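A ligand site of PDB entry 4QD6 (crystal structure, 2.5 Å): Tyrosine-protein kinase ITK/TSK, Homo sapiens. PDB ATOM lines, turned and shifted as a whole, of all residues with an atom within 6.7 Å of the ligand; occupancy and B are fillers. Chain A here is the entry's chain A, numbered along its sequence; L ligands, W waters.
N3 of the ligand is in hydrogen-bond range of O of Met 84, 2.7 Å away.
The backbone carbonyl oxygen of Glu 82 sits at hydrogen-bond distance from a nitrogen (N4) of the ligand, 3.3 Å away.
The backbone NH of Met 84 sits at hydrogen-bond distance from a nitrogen (N5) of the ligand, at 2.7 Å.
The side-chain amino group of Lys 37 lies within salt-bridge range of the side-chain carboxylate of Asp 146, at 3.1 Å.
O of Phe 81 lies within hydrogen-bond range of N of Ala 35, 2.8 Å away.
The backbone NH (N) of His 86 is in hydrogen-bond range of the backbone carbonyl oxygen (O) of Val 136 (3.0 Å).
The backbone NH of Gln 66 sits at hydrogen-bond distance from the side-chain carboxylate of Glu 82.
The backbone NH (N) of Val 136 sits at hydrogen-bond distance from the backbone carbonyl oxygen (O) of Gly 87 (3.0 Å).
The backbone carbonyl oxygen (O) of Glu 85 sits close to an oxygen (O2) of the ligand.
CB of Ala 35 touches N4 of the ligand, 3.5 Å away.
Lys 37 touches the ligand (CD to C25, 3.9 Å).
Val 65 touches the ligand.
Phe 81 touches the ligand (CG to C23, 3.1 Å).
Phe 83 touches the ligand (CE1 to N3, 3.5 Å).
His 86 touches the ligand.
N of Gly 87 touches C1 of the ligand, at 3.5 Å.
Leu 135 touches the ligand (CD1 to C14, 3.7 Å).
Hydrophobic or aromatic side chains that line the ligand: Ala 35, Val 65, Phe 81, Phe 83, Met 84 and Leu 135.
Water W2 lies within hydrogen-bond range of the side-chain carboxylate of Asp 146, the side-chain hydroxyl of Ser 145 and an oxygen (O3) of the ligand.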
ATOM      1  N   LYS A  33      24.213   5.679  22.150  1.00  0.00           N
ATOM      2  CA  LYS A  33      24.212   7.118  22.218  1.00  0.00           C
ATOM      3  C   LYS A  33      23.940   7.544  23.692  1.00  0.00           C
ATOM      4  O   LYS A  33      23.132   6.941  24.370  1.00  0.00           O
ATOM      5  CB  LYS A  33      23.138   7.627  21.277  1.00  0.00           C
ATOM      6  CG  LYS A  33      23.483   8.929  20.575  1.00  0.00           C
ATOM      7  CD  LYS A  33      22.528   9.252  19.433  1.00  0.00           C
ATOM      8  CE  LYS A  33      22.369   8.070  18.469  1.00  0.00           C
ATOM      9  NZ  LYS A  33      21.948   8.514  17.107  1.00  0.00           N
ATOM     10  N   VAL A  34      24.692   8.514  24.182  1.00  0.00           N
ATOM     11  CA  VAL A  34      24.548   8.988  25.545  1.00  0.00           C
ATOM     12  C   VAL A  34      24.723  10.492  25.656  1.00  0.00           C
ATOM     13  O   VAL A  34      25.231  11.146  24.733  1.00  0.00           O
ATOM     14  CB  VAL A  34      25.548   8.355  26.537  1.00  0.00           C
ATOM     15  CG1 VAL A  34      25.242   6.900  26.728  1.00  0.00           C
ATOM     16  CG2 VAL A  34      27.017   8.601  26.133  1.00  0.00           C
ATOM     17  N   ALA A  35      24.257  11.027  26.773  1.00  0.00           N
ATOM     18  CA  ALA A  35      24.378  12.428  27.070  1.00  0.00           C
ATOM     19  C   ALA A  35      25.317  12.404  28.240  1.00  0.00           C
ATOM     20  O   ALA A  35      25.147  11.605  29.171  1.00  0.00           O
ATOM     21  CB  ALA A  35      23.037  13.031  27.489  1.00  0.00           C
ATOM     22  N   ILE A  36      26.328  13.261  28.179  1.00  0.00           N
ATOM     23  CA  ILE A  36      27.381  13.251  29.145  1.00  0.00           C
ATOM     24  C   ILE A  36      27.359  14.596  29.816  1.00  0.00           C
ATOM     25  O   ILE A  36      27.527  15.617  29.140  1.00  0.00           O
ATOM     26  CB  ILE A  36      28.743  12.976  28.495  1.00  0.00           C
ATOM     27  CG1 ILE A  36      28.724  11.621  27.828  1.00  0.00           C
ATOM     28  CG2 ILE A  36      29.837  12.929  29.538  1.00  0.00           C
ATOM     29  CD1 ILE A  36      29.781  11.478  26.758  1.00  0.00           C
ATOM     30  N   LYS A  37      27.149  14.573  31.124  1.00  0.00           N
ATOM     31  CA  LYS A  37      27.032  15.779  31.929  1.00  0.00           C
ATOM     32  C   LYS A  37      28.308  15.989  32.738  1.00  0.00           C
ATOM     33  O   LYS A  37      28.564  15.301  33.748  1.00  0.00           O
ATOM     34  CB  LYS A  37      25.785  15.714  32.831  1.00  0.00           C
ATOM     35  CG  LYS A  37      25.382  17.058  33.436  1.00  0.00           C
ATOM     36  CD  LYS A  37      23.876  17.198  33.626  1.00  0.00           C
ATOM     37  CE  LYS A  37      23.512  18.590  34.112  1.00  0.00           C
ATOM     38  NZ  LYS A  37      22.091  18.721  34.548  1.00  0.00           N
ATOM     39  N   VAL A  65      14.450   9.809  32.729  1.00  0.00           N
ATOM     40  CA  VAL A  65      15.670   9.741  32.000  1.00  0.00           C
ATOM     41  C   VAL A  65      16.629   8.878  32.851  1.00  0.00           C
ATOM     42  O   VAL A  65      16.894   9.190  34.041  1.00  0.00           O
ATOM     43  CB  VAL A  65      16.142  11.185  31.797  1.00  0.00           C
ATOM     44  CG1 VAL A  65      17.634  11.314  31.912  1.00  0.00           C
ATOM     45  CG2 VAL A  65      15.675  11.669  30.455  1.00  0.00           C
ATOM     46  N   GLN A  66      17.119   7.783  32.263  1.00  0.00           N
ATOM     47  CA  GLN A  66      17.936   6.866  33.047  1.00  0.00           C
ATOM     48  C   GLN A  66      19.405   7.325  33.176  1.00  0.00           C
ATOM     49  O   GLN A  66      20.006   7.889  32.241  1.00  0.00           O
ATOM     50  CB  GLN A  66      17.770   5.420  32.549  1.00  0.00           C
ATOM     51  CG  GLN A  66      18.426   4.321  33.382  1.00  0.00           C
ATOM     52  CD  GLN A  66      18.531   2.960  32.645  1.00  0.00           C
ATOM     53  OE1 GLN A  66      19.171   2.025  33.141  1.00  0.00           O
ATOM     54  NE2 GLN A  66      17.910   2.861  31.459  1.00  0.00           N
ATOM     55  N   VAL A  80      26.797   9.862  33.075  1.00  0.00           N
ATOM     56  CA  VAL A  80      26.408   9.361  31.746  1.00  0.00           C
ATOM     57  C   VAL A  80      24.917   9.030  31.787  1.00  0.00           C
ATOM     58  O   VAL A  80      24.477   8.291  32.634  1.00  0.00           O
ATOM     59  CB  VAL A  80      27.231   8.111  31.318  1.00  0.00           C
ATOM     60  CG1 VAL A  80      26.872   7.636  29.904  1.00  0.00           C
ATOM     61  CG2 VAL A  80      28.711   8.393  31.385  1.00  0.00           C
ATOM     62  N   PHE A  81      24.159   9.578  30.833  1.00  0.00           N
ATOM     63  CA  PHE A  81      22.699   9.512  30.828  1.00  0.00           C
ATOM     64  C   PHE A  81      22.230   9.022  29.489  1.00  0.00           C
ATOM     65  O   PHE A  81      22.835   9.332  28.469  1.00  0.00           O
ATOM     66  CB  PHE A  81      22.091  10.899  30.989  1.00  0.00           C
ATOM     67  CG  PHE A  81      22.047  11.429  32.392  1.00  0.00           C
ATOM     68  CD1 PHE A  81      23.025  12.259  32.849  1.00  0.00           C
ATOM     69  CD2 PHE A  81      20.977  11.116  33.239  1.00  0.00           C
ATOM     70  CE1 PHE A  81      22.976  12.786  34.157  1.00  0.00           C
ATOM     71  CE2 PHE A  81      20.899  11.635  34.525  1.00  0.00           C
ATOM     72  CZ  PHE A  81      21.908  12.485  34.982  1.00  0.00           C
ATOM     73  N   GLU A  82      21.137   8.258  29.513  1.00  0.00           N
ATOM     74  CA  GLU A  82      20.340   7.979  28.361  1.00  0.00           C
ATOM     75  C   GLU A  82      20.361   9.188  27.455  1.00  0.00           C
ATOM     76  O   GLU A  82      20.255  10.347  27.929  1.00  0.00           O
ATOM     77  CB  GLU A  82      18.928   7.783  28.887  1.00  0.00           C
ATOM     78  CG  GLU A  82      17.774   7.775  27.906  1.00  0.00           C
ATOM     79  CD  GLU A  82      16.553   7.126  28.570  1.00  0.00           C
ATOM     80  OE1 GLU A  82      15.639   6.667  27.826  1.00  0.00           O
ATOM     81  OE2 GLU A  82      16.525   7.053  29.845  1.00  0.00           O
ATOM     82  N   PHE A  83      20.507   8.950  26.163  1.00  0.00           N
ATOM     83  CA  PHE A  83      20.448  10.080  25.240  1.00  0.00           C
ATOM     84  C   PHE A  83      19.039  10.252  24.716  1.00  0.00           C
ATOM     85  O   PHE A  83      18.456   9.332  24.195  1.00  0.00           O
ATOM     86  CB  PHE A  83      21.386   9.919  24.032  1.00  0.00           C
ATOM     87  CG  PHE A  83      21.224  11.018  23.006  1.00  0.00           C
ATOM     88  CD1 PHE A  83      21.637  12.328  23.279  1.00  0.00           C
ATOM     89  CD2 PHE A  83      20.617  10.771  21.793  1.00  0.00           C
ATOM     90  CE1 PHE A  83      21.463  13.349  22.359  1.00  0.00           C
ATOM     91  CE2 PHE A  83      20.467  11.794  20.853  1.00  0.00           C
ATOM     92  CZ  PHE A  83      20.884  13.083  21.133  1.00  0.00           C
ATOM     93  N   MET A  84      18.541  11.456  24.766  1.00  0.00           N
ATOM     94  CA  MET A  84      17.167  11.748  24.367  1.00  0.00           C
ATOM     95  C   MET A  84      17.143  12.497  23.046  1.00  0.00           C
ATOM     96  O   MET A  84      17.519  13.672  22.967  1.00  0.00           O
ATOM     97  CB  MET A  84      16.416  12.538  25.453  1.00  0.00           C
ATOM     98  CG  MET A  84      16.102  11.746  26.732  1.00  0.00           C
ATOM     99  SD  MET A  84      15.208  10.222  26.426  1.00  0.00           S
ATOM    100  CE  MET A  84      13.644  10.813  25.802  1.00  0.00           C
ATOM    101  N   GLU A  85      16.695  11.773  22.024  1.00  0.00           N
ATOM    102  CA  GLU A  85      16.608  12.206  20.638  1.00  0.00           C
ATOM    103  C   GLU A  85      16.475  13.693  20.341  1.00  0.00           C
ATOM    104  O   GLU A  85      17.364  14.279  19.759  1.00  0.00           O
ATOM    105  CB  GLU A  85      15.396  11.520  20.026  1.00  0.00           C
ATOM    106  CG  GLU A  85      15.523  11.153  18.571  1.00  0.00           C
ATOM    107  CD  GLU A  85      16.296   9.866  18.396  1.00  0.00           C
ATOM    108  OE1 GLU A  85      15.636   8.840  18.113  1.00  0.00           O
ATOM    109  OE2 GLU A  85      17.533   9.902  18.572  1.00  0.00           O
ATOM    110  N   HIS A  86      15.326  14.277  20.727  1.00  0.00           N
ATOM    111  CA  HIS A  86      14.897  15.615  20.298  1.00  0.00           C
ATOM    112  C   HIS A  86      14.982  16.690  21.369  1.00  0.00           C
ATOM    113  O   HIS A  86      14.400  17.771  21.195  1.00  0.00           O
ATOM    114  CB  HIS A  86      13.459  15.585  19.802  1.00  0.00           C
ATOM    115  CG  HIS A  86      13.174  14.464  18.849  1.00  0.00           C
ATOM    116  ND1 HIS A  86      13.663  14.422  17.567  1.00  0.00           N
ATOM    117  CD2 HIS A  86      12.428  13.336  19.000  1.00  0.00           C
ATOM    118  CE1 HIS A  86      13.247  13.317  16.967  1.00  0.00           C
ATOM    119  NE2 HIS A  86      12.507  12.640  17.818  1.00  0.00           N
ATOM    120  N   GLY A  87      15.682  16.413  22.463  1.00  0.00           N
ATOM    121  CA  GLY A  87      15.994  17.461  23.455  1.00  0.00           C
ATOM    122  C   GLY A  87      14.755  18.044  24.134  1.00  0.00           C
ATOM    123  O   GLY A  87      13.691  17.457  24.075  1.00  0.00           O
ATOM    124  N   CYS A  88      14.890  19.213  24.731  1.00  0.00           N
ATOM    125  CA  CYS A  88      13.962  19.607  25.759  1.00  0.00           C
ATOM    126  C   CYS A  88      12.547  20.006  25.287  1.00  0.00           C
ATOM    127  O   CYS A  88      12.358  20.672  24.282  1.00  0.00           O
ATOM    128  CB  CYS A  88      14.584  20.603  26.744  1.00  0.00           C
ATOM    129  SG  CYS A  88      14.859  22.286  26.183  1.00  0.00           S
ATOM    130  N   ARG A 132      11.178  22.758  30.479  1.00  0.00           N
ATOM    131  CA  ARG A 132      12.593  22.869  30.149  1.00  0.00           C
ATOM    132  C   ARG A 132      13.406  21.719  30.831  1.00  0.00           C
ATOM    133  O   ARG A 132      14.562  21.474  30.479  1.00  0.00           O
ATOM    134  CB  ARG A 132      13.102  24.248  30.562  1.00  0.00           C
ATOM    135  CG  ARG A 132      13.412  24.357  32.053  1.00  0.00           C
ATOM    136  CD  ARG A 132      13.777  25.763  32.534  1.00  0.00           C
ATOM    137  NE  ARG A 132      12.763  26.204  33.481  1.00  0.00           N
ATOM    138  CZ  ARG A 132      12.819  25.977  34.798  1.00  0.00           C
ATOM    139  NH1 ARG A 132      13.859  25.346  35.344  1.00  0.00           N
ATOM    140  NH2 ARG A 132      11.828  26.390  35.583  1.00  0.00           N
ATOM    141  N   ASN A 133      12.812  21.022  31.806  1.00  0.00           N
ATOM    142  CA  ASN A 133      13.485  19.915  32.459  1.00  0.00           C
ATOM    143  C   ASN A 133      12.944  18.560  31.996  1.00  0.00           C
ATOM    144  O   ASN A 133      13.159  17.547  32.664  1.00  0.00           O
ATOM    145  CB  ASN A 133      13.416  20.056  33.972  1.00  0.00           C
ATOM    146  CG  ASN A 133      14.360  21.112  34.491  1.00  0.00           C
ATOM    147  OD1 ASN A 133      15.544  21.105  34.168  1.00  0.00           O
ATOM    148  ND2 ASN A 133      13.840  22.039  35.325  1.00  0.00           N
ATOM    149  N   CYS A 134      12.229  18.538  30.875  1.00  0.00           N
ATOM    150  CA  CYS A 134      11.715  17.302  30.292  1.00  0.00           C
ATOM    151  C   CYS A 134      12.278  17.166  28.921  1.00  0.00           C
ATOM    152  O   CYS A 134      12.420  18.148  28.230  1.00  0.00           O
ATOM    153  CB  CYS A 134      10.198  17.304  30.175  1.00  0.00           C
ATOM    154  SG  CYS A 134       9.409  17.314  31.786  1.00  0.00           S
ATOM    155  N   LEU A 135      12.581  15.938  28.536  1.00  0.00           N
ATOM    156  CA  LEU A 135      13.247  15.694  27.256  1.00  0.00           C
ATOM    157  C   LEU A 135      12.305  14.839  26.450  1.00  0.00           C
ATOM    158  O   LEU A 135      11.519  14.114  27.014  1.00  0.00           O
ATOM    159  CB  LEU A 135      14.603  15.024  27.482  1.00  0.00           C
ATOM    160  CG  LEU A 135      15.502  15.827  28.452  1.00  0.00           C
ATOM    161  CD1 LEU A 135      16.560  15.023  29.172  1.00  0.00           C
ATOM    162  CD2 LEU A 135      16.176  16.975  27.759  1.00  0.00           C
ATOM    163  N   VAL A 136      12.338  15.015  25.138  1.00  0.00           N
ATOM    164  CA  VAL A 136      11.592  14.210  24.173  1.00  0.00           C
ATOM    165  C   VAL A 136      12.497  13.160  23.470  1.00  0.00           C
ATOM    166  O   VAL A 136      13.600  13.454  23.007  1.00  0.00           O
ATOM    167  CB  VAL A 136      11.042  15.117  23.080  1.00  0.00           C
ATOM    168  CG1 VAL A 136       9.997  14.372  22.290  1.00  0.00           C
ATOM    169  CG2 VAL A 136      10.415  16.330  23.708  1.00  0.00           C
ATOM    170  N   SER A 145      13.492  14.768  33.602  1.00  0.00           N
ATOM    171  CA  SER A 145      14.877  14.709  33.960  1.00  0.00           C
ATOM    172  C   SER A 145      15.240  15.687  35.077  1.00  0.00           C
ATOM    173  O   SER A 145      14.354  16.336  35.645  1.00  0.00           O
ATOM    174  CB  SER A 145      15.756  14.802  32.720  1.00  0.00           C
ATOM    175  OG  SER A 145      15.752  16.135  32.307  1.00  0.00           O
ATOM    176  N   ASP A 146      16.521  15.731  35.419  1.00  0.00           N
ATOM    177  CA  ASP A 146      17.050  16.582  36.462  1.00  0.00           C
ATOM    178  C   ASP A 146      16.315  16.492  37.797  1.00  0.00           C
ATOM    179  O   ASP A 146      16.084  17.516  38.493  1.00  0.00           O
ATOM    180  CB  ASP A 146      17.226  18.021  35.965  1.00  0.00           C
ATOM    181  CG  ASP A 146      18.410  18.159  35.018  1.00  0.00           C
ATOM    182  OD1 ASP A 146      19.340  17.314  35.074  1.00  0.00           O
ATOM    183  OD2 ASP A 146      18.391  19.110  34.215  1.00  0.00           O
HETATM  184  C1  LIG L   1      19.196  16.446  22.395  1.00  0.00           C
HETATM  185  C2  LIG L   1      19.391  17.681  21.800  1.00  0.00           C
HETATM  186  C3  LIG L   1      19.791  18.763  22.577  1.00  0.00           C
HETATM  187  C4  LIG L   1      19.993  18.570  23.968  1.00  0.00           C
HETATM  188  N1  LIG L   1      19.793  17.368  24.525  1.00  0.00           N
HETATM  189  C5  LIG L   1      19.392  16.324  23.773  1.00  0.00           C
HETATM  190  S1  LIG L   1      19.157  17.779  20.209  1.00  0.00           S
HETATM  191  C6  LIG L   1      20.124  16.811  19.337  1.00  0.00           C
HETATM  192  C7  LIG L   1      21.518  16.948  19.341  1.00  0.00           C
HETATM  193  C8  LIG L   1      22.294  16.095  18.563  1.00  0.00           C
HETATM  194  C9  LIG L   1      21.710  15.107  17.758  1.00  0.00           C
HETATM  195  C10 LIG L   1      20.318  14.971  17.732  1.00  0.00           C
HETATM  196  C11 LIG L   1      19.545  15.823  18.519  1.00  0.00           C
HETATM  197  O1  LIG L   1      19.394  19.139  19.811  1.00  0.00           O
HETATM  198  O2  LIG L   1      17.828  17.337  19.833  1.00  0.00           O
HETATM  199  N2  LIG L   1      20.378  19.526  24.838  1.00  0.00           N
HETATM  200  N3  LIG L   1      19.232  15.148  24.380  1.00  0.00           N
HETATM  201  C12 LIG L   1      19.532  14.979  25.693  1.00  0.00           C
HETATM  202  C13 LIG L   1      19.916  15.739  26.774  1.00  0.00           C
HETATM  203  C14 LIG L   1      19.953  14.802  27.786  1.00  0.00           C
HETATM  204  N4  LIG L   1      19.617  13.589  27.415  1.00  0.00           N
HETATM  205  N5  LIG L   1      19.357  13.730  26.064  1.00  0.00           N
HETATM  206  C15 LIG L   1      20.216  19.361  26.288  1.00  0.00           C
HETATM  207  C16 LIG L   1      18.849  19.896  26.691  1.00  0.00           C
HETATM  208  C17 LIG L   1      18.656  19.817  28.203  1.00  0.00           C
HETATM  209  C18 LIG L   1      19.755  20.520  29.022  1.00  0.00           C
HETATM  210  C19 LIG L   1      21.166  20.222  28.523  1.00  0.00           C
HETATM  211  C20 LIG L   1      21.286  20.171  27.009  1.00  0.00           C
HETATM  212  O3  LIG L   1      19.660  20.060  30.380  1.00  0.00           O
HETATM  213  C21 LIG L   1      20.262  14.795  29.214  1.00  0.00           C
HETATM  214  C22 LIG L   1      19.937  13.654  29.921  1.00  0.00           C
HETATM  215  C23 LIG L   1      20.208  13.673  31.281  1.00  0.00           C
HETATM  216  C24 LIG L   1      20.819  14.784  31.913  1.00  0.00           C
HETATM  217  C25 LIG L   1      21.148  15.899  31.159  1.00  0.00           C
HETATM  218  C26 LIG L   1      20.857  15.922  29.778  1.00  0.00           C
HETATM  219  O   HOH W   1      19.110  17.625  16.276  1.00  0.00           O
HETATM  220  O   HOH W   2      17.973  18.159  32.046  1.00  0.00           O
